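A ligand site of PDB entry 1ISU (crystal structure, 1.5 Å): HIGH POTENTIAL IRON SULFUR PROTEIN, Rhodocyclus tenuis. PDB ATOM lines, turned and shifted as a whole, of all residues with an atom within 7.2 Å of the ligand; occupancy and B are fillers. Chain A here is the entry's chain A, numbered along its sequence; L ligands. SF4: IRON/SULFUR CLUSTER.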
ATOM      1  N   PHE A  10      -0.871  16.760  20.327  1.00  0.00           N
ATOM      2  CA  PHE A  10       0.564  16.711  19.998  1.00  0.00           C
ATOM      3  C   PHE A  10       1.029  15.430  19.298  1.00  0.00           C
ATOM      4  O   PHE A  10       2.226  15.161  19.193  1.00  0.00           O
ATOM      5  CB  PHE A  10       1.393  17.012  21.280  1.00  0.00           C
ATOM      6  CG  PHE A  10       1.129  18.416  21.806  1.00  0.00           C
ATOM      7  CD1 PHE A  10       1.581  19.524  21.084  1.00  0.00           C
ATOM      8  CD2 PHE A  10       0.398  18.629  22.980  1.00  0.00           C
ATOM      9  CE1 PHE A  10       1.326  20.811  21.556  1.00  0.00           C
ATOM     10  CE2 PHE A  10       0.128  19.907  23.473  1.00  0.00           C
ATOM     11  CZ  PHE A  10       0.614  20.988  22.735  1.00  0.00           C
ATOM     12  N   TYR A  12       1.107  12.291  20.153  1.00  0.00           N
ATOM     13  CA  TYR A  12       1.913  11.433  20.977  1.00  0.00           C
ATOM     14  C   TYR A  12       1.910   9.990  20.371  1.00  0.00           C
ATOM     15  O   TYR A  12       0.910   9.487  19.839  1.00  0.00           O
ATOM     16  CB  TYR A  12       1.324  11.426  22.396  1.00  0.00           C
ATOM     17  CG  TYR A  12       2.011  10.426  23.268  1.00  0.00           C
ATOM     18  CD1 TYR A  12       1.515   9.116  23.314  1.00  0.00           C
ATOM     19  CD2 TYR A  12       3.139  10.775  24.010  1.00  0.00           C
ATOM     20  CE1 TYR A  12       2.136   8.143  24.107  1.00  0.00           C
ATOM     21  CE2 TYR A  12       3.766   9.818  24.814  1.00  0.00           C
ATOM     22  CZ  TYR A  12       3.253   8.513  24.842  1.00  0.00           C
ATOM     23  OH  TYR A  12       3.885   7.587  25.617  1.00  0.00           O
ATOM     24  N   GLN A  13       3.061   9.345  20.449  1.00  0.00           N
ATOM     25  CA  GLN A  13       3.233   7.994  19.948  1.00  0.00           C
ATOM     26  C   GLN A  13       4.076   7.263  20.991  1.00  0.00           C
ATOM     27  O   GLN A  13       4.828   7.891  21.746  1.00  0.00           O
ATOM     28  CB  GLN A  13       3.803   7.897  18.543  1.00  0.00           C
ATOM     29  CG  GLN A  13       5.103   8.661  18.428  1.00  0.00           C
ATOM     30  CD  GLN A  13       5.634   8.647  17.033  1.00  0.00           C
ATOM     31  OE1 GLN A  13       4.924   9.003  16.079  1.00  0.00           O
ATOM     32  NE2 GLN A  13       6.886   8.232  16.891  1.00  0.00           N
ATOM     33  N   LYS A  20      14.560  10.520  18.736  1.00  0.00           N
ATOM     34  CA  LYS A  20      14.050  11.468  19.703  1.00  0.00           C
ATOM     35  C   LYS A  20      13.010  10.783  20.577  1.00  0.00           C
ATOM     36  O   LYS A  20      12.049  10.222  20.055  1.00  0.00           O
ATOM     37  CB  LYS A  20      13.400  12.663  19.026  1.00  0.00           C
ATOM     38  CG  LYS A  20      14.294  13.412  18.044  1.00  0.00           C
ATOM     39  CD  LYS A  20      13.454  14.233  17.071  1.00  0.00           C
ATOM     40  CE  LYS A  20      14.267  15.207  16.208  1.00  0.00           C
ATOM     41  NZ  LYS A  20      13.511  15.665  15.020  1.00  0.00           N
ATOM     42  N   LYS A  21      13.168  10.838  21.885  1.00  0.00           N
ATOM     43  CA  LYS A  21      12.209  10.199  22.761  1.00  0.00           C
ATOM     44  C   LYS A  21      12.029  10.981  24.035  1.00  0.00           C
ATOM     45  O   LYS A  21      12.881  11.776  24.404  1.00  0.00           O
ATOM     46  CB  LYS A  21      12.600   8.770  23.049  1.00  0.00           C
ATOM     47  CG  LYS A  21      13.942   8.659  23.741  1.00  0.00           C
ATOM     48  CD  LYS A  21      14.386   7.224  23.844  1.00  0.00           C
ATOM     49  CE  LYS A  21      15.590   7.076  24.735  1.00  0.00           C
ATOM     50  NZ  LYS A  21      16.823   7.557  24.094  1.00  0.00           N
ATOM     51  N   CYS A  22      10.911  10.742  24.707  1.00  0.00           N
ATOM     52  CA  CYS A  22      10.578  11.414  25.946  1.00  0.00           C
ATOM     53  C   CYS A  22      11.685  11.482  26.977  1.00  0.00           C
ATOM     54  O   CYS A  22      11.888  12.527  27.598  1.00  0.00           O
ATOM     55  CB  CYS A  22       9.311  10.854  26.611  1.00  0.00           C
ATOM     56  SG  CYS A  22       7.833  10.943  25.561  1.00  0.00           S
ATOM     57  N   SER A  23      12.389  10.377  27.221  1.00  0.00           N
ATOM     58  CA  SER A  23      13.451  10.402  28.229  1.00  0.00           C
ATOM     59  C   SER A  23      14.588  11.419  27.888  1.00  0.00           C
ATOM     60  O   SER A  23      15.359  11.827  28.750  1.00  0.00           O
ATOM     61  CB  SER A  23      13.982   9.010  28.538  1.00  0.00           C
ATOM     62  OG  SER A  23      14.571   8.470  27.378  1.00  0.00           O
ATOM     63  N   GLY A  24      14.672  11.830  26.624  1.00  0.00           N
ATOM     64  CA  GLY A  24      15.701  12.795  26.268  1.00  0.00           C
ATOM     65  C   GLY A  24      15.097  14.195  26.023  1.00  0.00           C
ATOM     66  O   GLY A  24      15.765  15.074  25.484  1.00  0.00           O
ATOM     67  N   CYS A  25      13.839  14.392  26.411  1.00  0.00           N
ATOM     68  CA  CYS A  25      13.108  15.665  26.214  1.00  0.00           C
ATOM     69  C   CYS A  25      13.064  16.526  27.451  1.00  0.00           C
ATOM     70  O   CYS A  25      12.880  16.023  28.552  1.00  0.00           O
ATOM     71  CB  CYS A  25      11.670  15.301  25.784  1.00  0.00           C
ATOM     72  SG  CYS A  25      10.576  16.723  25.560  1.00  0.00           S
ATOM     73  N   ALA A  26      13.232  17.817  27.292  1.00  0.00           N
ATOM     74  CA  ALA A  26      13.207  18.713  28.448  1.00  0.00           C
ATOM     75  C   ALA A  26      11.851  18.829  29.171  1.00  0.00           C
ATOM     76  O   ALA A  26      11.800  19.287  30.315  1.00  0.00           O
ATOM     77  CB  ALA A  26      13.677  20.092  28.023  1.00  0.00           C
ATOM     78  N   GLN A  27      10.749  18.449  28.515  1.00  0.00           N
ATOM     79  CA  GLN A  27       9.412  18.543  29.113  1.00  0.00           C
ATOM     80  C   GLN A  27       9.027  17.320  29.948  1.00  0.00           C
ATOM     81  O   GLN A  27       8.026  17.331  30.656  1.00  0.00           O
ATOM     82  CB  GLN A  27       8.308  18.718  28.038  1.00  0.00           C
ATOM     83  CG  GLN A  27       8.438  19.968  27.132  1.00  0.00           C
ATOM     84  CD  GLN A  27       8.077  21.309  27.801  1.00  0.00           C
ATOM     85  OE1 GLN A  27       8.091  21.426  29.038  1.00  0.00           O
ATOM     86  NE2 GLN A  27       7.789  22.312  26.975  1.00  0.00           N
ATOM     87  N   PHE A  28       9.816  16.265  29.835  1.00  0.00           N
ATOM     88  CA  PHE A  28       9.549  15.030  30.553  1.00  0.00           C
ATOM     89  C   PHE A  28       9.807  15.123  32.047  1.00  0.00           C
ATOM     90  O   PHE A  28      10.742  15.773  32.490  1.00  0.00           O
ATOM     91  CB  PHE A  28      10.474  13.911  30.021  1.00  0.00           C
ATOM     92  CG  PHE A  28      10.140  12.485  30.426  1.00  0.00           C
ATOM     93  CD1 PHE A  28       8.876  11.914  30.205  1.00  0.00           C
ATOM     94  CD2 PHE A  28      11.136  11.727  31.023  1.00  0.00           C
ATOM     95  CE1 PHE A  28       8.564  10.604  30.540  1.00  0.00           C
ATOM     96  CE2 PHE A  28      10.849  10.411  31.373  1.00  0.00           C
ATOM     97  CZ  PHE A  28       9.589   9.857  31.125  1.00  0.00           C
ATOM     98  N   VAL A  29       8.957  14.438  32.822  1.00  0.00           N
ATOM     99  CA  VAL A  29       9.066  14.350  34.289  1.00  0.00           C
ATOM    100  C   VAL A  29       9.242  12.830  34.508  1.00  0.00           C
ATOM    101  O   VAL A  29       8.275  12.081  34.409  1.00  0.00           O
ATOM    102  CB  VAL A  29       7.834  14.871  35.039  1.00  0.00           C
ATOM    103  CG1 VAL A  29       8.097  14.821  36.536  1.00  0.00           C
ATOM    104  CG2 VAL A  29       7.526  16.295  34.623  1.00  0.00           C
ATOM    105  N   GLY A  39       5.592  11.695  33.521  1.00  0.00           N
ATOM    106  CA  GLY A  39       4.689  12.772  33.202  1.00  0.00           C
ATOM    107  C   GLY A  39       5.332  13.694  32.172  1.00  0.00           C
ATOM    108  O   GLY A  39       6.458  13.459  31.723  1.00  0.00           O
ATOM    109  N   CYS A  40       4.579  14.714  31.784  1.00  0.00           N
ATOM    110  CA  CYS A  40       5.031  15.686  30.801  1.00  0.00           C
ATOM    111  C   CYS A  40       4.373  17.059  31.027  1.00  0.00           C
ATOM    112  O   CYS A  40       3.160  17.145  31.277  1.00  0.00           O
ATOM    113  CB  CYS A  40       4.705  15.138  29.396  1.00  0.00           C
ATOM    114  SG  CYS A  40       4.992  16.329  28.070  1.00  0.00           S
ATOM    115  N   LYS A  41       5.168  18.135  30.944  1.00  0.00           N
ATOM    116  CA  LYS A  41       4.638  19.475  31.151  1.00  0.00           C
ATOM    117  C   LYS A  41       3.631  19.909  30.110  1.00  0.00           C
ATOM    118  O   LYS A  41       2.751  20.717  30.390  1.00  0.00           O
ATOM    119  CB  LYS A  41       5.727  20.515  31.316  1.00  0.00           C
ATOM    120  CG  LYS A  41       6.658  20.087  32.444  1.00  0.00           C
ATOM    121  CD  LYS A  41       7.007  21.204  33.434  1.00  0.00           C
ATOM    122  CE  LYS A  41       8.469  21.661  33.312  1.00  0.00           C
ATOM    123  NZ  LYS A  41       8.999  22.336  34.520  1.00  0.00           N
ATOM    124  N   VAL A  42       3.741  19.360  28.920  1.00  0.00           N
ATOM    125  CA  VAL A  42       2.845  19.713  27.828  1.00  0.00           C
ATOM    126  C   VAL A  42       1.560  18.871  27.736  1.00  0.00           C
ATOM    127  O   VAL A  42       0.658  19.200  26.976  1.00  0.00           O
ATOM    128  CB  VAL A  42       3.681  19.612  26.548  1.00  0.00           C
ATOM    129  CG1 VAL A  42       2.836  19.501  25.276  1.00  0.00           C
ATOM    130  CG2 VAL A  42       4.715  20.729  26.464  1.00  0.00           C
ATOM    131  N   ILE A  43       1.492  17.790  28.512  1.00  0.00           N
ATOM    132  CA  ILE A  43       0.322  16.879  28.532  1.00  0.00           C
ATOM    133  C   ILE A  43      -0.097  16.721  29.972  1.00  0.00           C
ATOM    134  O   ILE A  43       0.151  15.695  30.596  1.00  0.00           O
ATOM    135  CB  ILE A  43       0.690  15.534  27.884  1.00  0.00           C
ATOM    136  CG1 ILE A  43       1.229  15.791  26.478  1.00  0.00           C
ATOM    137  CG2 ILE A  43      -0.527  14.610  27.801  1.00  0.00           C
ATOM    138  CD1 ILE A  43       1.556  14.529  25.712  1.00  0.00           C
ATOM    139  N   ILE A  49       3.110   8.559  30.453  1.00  0.00           N
ATOM    140  CA  ILE A  49       3.982   8.963  29.376  1.00  0.00           C
ATOM    141  C   ILE A  49       5.163   7.978  29.324  1.00  0.00           C
ATOM    142  O   ILE A  49       5.896   7.839  30.300  1.00  0.00           O
ATOM    143  CB  ILE A  49       4.473  10.422  29.539  1.00  0.00           C
ATOM    144  CG1 ILE A  49       3.299  11.411  29.580  1.00  0.00           C
ATOM    145  CG2 ILE A  49       5.408  10.805  28.405  1.00  0.00           C
ATOM    146  CD1 ILE A  49       2.480  11.434  28.303  1.00  0.00           C
ATOM    147  N   ALA A  50       5.342   7.279  28.206  1.00  0.00           N
ATOM    148  CA  ALA A  50       6.443   6.321  28.065  1.00  0.00           C
ATOM    149  C   ALA A  50       7.805   7.002  27.819  1.00  0.00           C
ATOM    150  O   ALA A  50       7.916   7.891  26.986  1.00  0.00           O
ATOM    151  CB  ALA A  50       6.148   5.363  26.927  1.00  0.00           C
ATOM    152  N   PRO A  51       8.848   6.583  28.526  1.00  0.00           N
ATOM    153  CA  PRO A  51      10.172   7.166  28.330  1.00  0.00           C
ATOM    154  C   PRO A  51      10.674   7.001  26.875  1.00  0.00           C
ATOM    155  O   PRO A  51      11.487   7.793  26.387  1.00  0.00           O
ATOM    156  CB  PRO A  51      11.081   6.500  29.355  1.00  0.00           C
ATOM    157  CG  PRO A  51      10.276   5.384  30.015  1.00  0.00           C
ATOM    158  CD  PRO A  51       8.822   5.572  29.618  1.00  0.00           C
ATOM    159  N   GLY A  53       8.600   7.053  24.227  1.00  0.00           N
ATOM    160  CA  GLY A  53       7.602   7.679  23.360  1.00  0.00           C
ATOM    161  C   GLY A  53       8.131   8.982  22.759  1.00  0.00           C
ATOM    162  O   GLY A  53       9.309   9.311  22.879  1.00  0.00           O
ATOM    163  N   TYR A  54       7.237   9.707  22.099  1.00  0.00           N
ATOM    164  CA  TYR A  54       7.564  10.958  21.455  1.00  0.00           C
ATOM    165  C   TYR A  54       6.285  11.738  21.139  1.00  0.00           C
ATOM    166  O   TYR A  54       5.204  11.167  20.988  1.00  0.00           O
ATOM    167  CB  TYR A  54       8.283  10.611  20.077  1.00  0.00           C
ATOM    168  CG  TYR A  54       8.432  11.795  19.128  1.00  0.00           C
ATOM    169  CD1 TYR A  54       9.559  12.612  19.266  1.00  0.00           C
ATOM    170  CD2 TYR A  54       7.442  12.079  18.187  1.00  0.00           C
ATOM    171  CE1 TYR A  54       9.726  13.713  18.428  1.00  0.00           C
ATOM    172  CE2 TYR A  54       7.599  13.180  17.352  1.00  0.00           C
ATOM    173  CZ  TYR A  54       8.728  13.991  17.498  1.00  0.00           C
ATOM    174  OH  TYR A  54       8.881  15.057  16.663  1.00  0.00           O
ATOM    175  N   CYS A  55       6.415  13.039  21.022  1.00  0.00           N
ATOM    176  CA  CYS A  55       5.337  13.927  20.664  1.00  0.00           C
ATOM    177  C   CYS A  55       5.912  15.101  19.874  1.00  0.00           C
ATOM    178  O   CYS A  55       7.127  15.330  19.919  1.00  0.00           O
ATOM    179  CB  CYS A  55       4.246  14.258  21.708  1.00  0.00           C
ATOM    180  SG  CYS A  55       4.626  15.733  22.660  1.00  0.00           S
ATOM    181  N   ASP A  56       5.078  15.819  19.140  1.00  0.00           N
ATOM    182  CA  ASP A  56       5.565  16.943  18.359  1.00  0.00           C
ATOM    183  C   ASP A  56       6.242  18.035  19.196  1.00  0.00           C
ATOM    184  O   ASP A  56       7.017  18.821  18.661  1.00  0.00           O
ATOM    185  CB  ASP A  56       4.452  17.614  17.543  1.00  0.00           C
ATOM    186  CG  ASP A  56       3.779  16.756  16.511  1.00  0.00           C
ATOM    187  OD1 ASP A  56       4.534  15.789  16.050  1.00  0.00           O
ATOM    188  OD2 ASP A  56       2.638  16.959  16.152  1.00  0.00           O
ATOM    189  N   ALA A  57       5.939  18.117  20.485  1.00  0.00           N
ATOM    190  CA  ALA A  57       6.522  19.147  21.349  1.00  0.00           C
ATOM    191  C   ALA A  57       7.934  18.822  21.857  1.00  0.00           C
ATOM    192  O   ALA A  57       8.497  19.545  22.681  1.00  0.00           O
ATOM    193  CB  ALA A  57       5.572  19.471  22.496  1.00  0.00           C
ATOM    194  N   PHE A  58       8.494  17.727  21.369  1.00  0.00           N
ATOM    195  CA  PHE A  58       9.814  17.329  21.791  1.00  0.00           C
ATOM    196  C   PHE A  58      10.873  18.459  21.712  1.00  0.00           C
ATOM    197  O   PHE A  58      10.937  19.199  20.735  1.00  0.00           O
ATOM    198  CB  PHE A  58      10.286  16.149  20.923  1.00  0.00           C
ATOM    199  CG  PHE A  58      11.744  15.778  21.178  1.00  0.00           C
ATOM    200  CD1 PHE A  58      12.084  14.898  22.203  1.00  0.00           C
ATOM    201  CD2 PHE A  58      12.786  16.292  20.403  1.00  0.00           C
ATOM    202  CE1 PHE A  58      13.422  14.541  22.446  1.00  0.00           C
ATOM    203  CE2 PHE A  58      14.117  15.925  20.627  1.00  0.00           C
ATOM    204  CZ  PHE A  58      14.453  15.062  21.667  1.00  0.00           C
ATOM    205  N   ILE A  59      11.700  18.562  22.749  1.00  0.00           N
ATOM    206  CA  ILE A  59      12.773  19.558  22.821  1.00  0.00           C
ATOM    207  C   ILE A  59      13.896  18.904  23.569  1.00  0.00           C
ATOM    208  O   ILE A  59      13.723  18.457  24.711  1.00  0.00           O
ATOM    209  CB  ILE A  59      12.347  20.915  23.298  1.00  0.00           C
ATOM    210  CG1 ILE A  59      13.558  21.819  23.431  1.00  0.00           C
ATOM    211  CG2 ILE A  59      11.501  20.858  24.574  1.00  0.00           C
ATOM    212  CD1 ILE A  59      13.164  23.285  23.495  1.00  0.00           C
HETATM  213 FE1  SF4 L   1       7.380  13.157  25.435  1.00  0.00          FE
HETATM  214 FE2  SF4 L   1       8.538  15.663  25.368  1.00  0.00          FE
HETATM  215 FE3  SF4 L   1       6.133  15.268  26.626  1.00  0.00          FE
HETATM  216 FE4  SF4 L   1       6.247  15.117  23.974  1.00  0.00          FE
HETATM  217  S1  SF4 L   1       6.798  16.958  25.169  1.00  0.00           S
HETATM  218  S2  SF4 L   1       5.263  13.610  25.369  1.00  0.00           S
HETATM  219  S3  SF4 L   1       8.367  14.182  23.600  1.00  0.00           S
HETATM  220  S4  SF4 L   1       8.165  14.359  27.196  1.00  0.00           S
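The side-chain sulfur of Cys 40 is bound to an iron atom (FE3) of the ligand.
The backbone NH (N) of Cys 55 sits close to a sulfur (S3) of the ligand, at 3.4 Å.
The side-chain sulfur (SG) of Cys 55 is bound to an iron atom (FE4) of the ligand (2.2 Å).
SG of Cys 22 is bound to FE1 of the ligand (2.3 Å).
An iron atom (FE2) of the ligand is bound by the side-chain sulfur of Cys 25 (2.3 Å).
The backbone NH (N) of Phe 28 sits close to a sulfur (S4) of the ligand, at 3.7 Å.
The side-chain sulfur (SG) of Cys 55 sits close to the backbone NH (N) of Ala 57 (3.5 Å).
The side-chain sulfur (SG) of Cys 22 lies close to the backbone NH (N) of Tyr 54, at 3.7 Å.
The backbone NH of Cys 22 lies within hydrogen-bond range of the backbone carbonyl oxygen of Gly 53, 2.8 Å away.
O of Ala 50 lies close to SG of Cys 22, 3.4 Å away.
N of Cys 22 is in hydrogen-bond range of O of Pro 51, 3.4 Å away.
SG of Cys 25 lies close to N of Ile 59, at 3.5 Å.
The backbone NH of Lys 41 lies within hydrogen-bond range of the backbone carbonyl oxygen of Gln 27, 3.0 Å away.
The side-chain hydroxyl of Tyr 12 sits at hydrogen-bond distance from the backbone NH of Ala 50, 3.0 Å away.
Tyr 12 touches the ligand (CD2 to S2, 3.8 Å).
Gln 27 touches the ligand (CB to S1, 3.7 Å).
Ile 43 touches the ligand (CD1 to S2, 3.8 Å).
Tyr 54 touches the ligand (CA to S3, 3.95 Å).
Ala 57 touches the ligand (CB to S1, 3.9 Å).
CB of Phe 58 touches S3 of the ligand, 3.8 Å away.
Hydrophobic or aromatic side chains that line the ligand: Tyr 12, Phe 28, Ile 43, Ala 57 and Phe 58.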
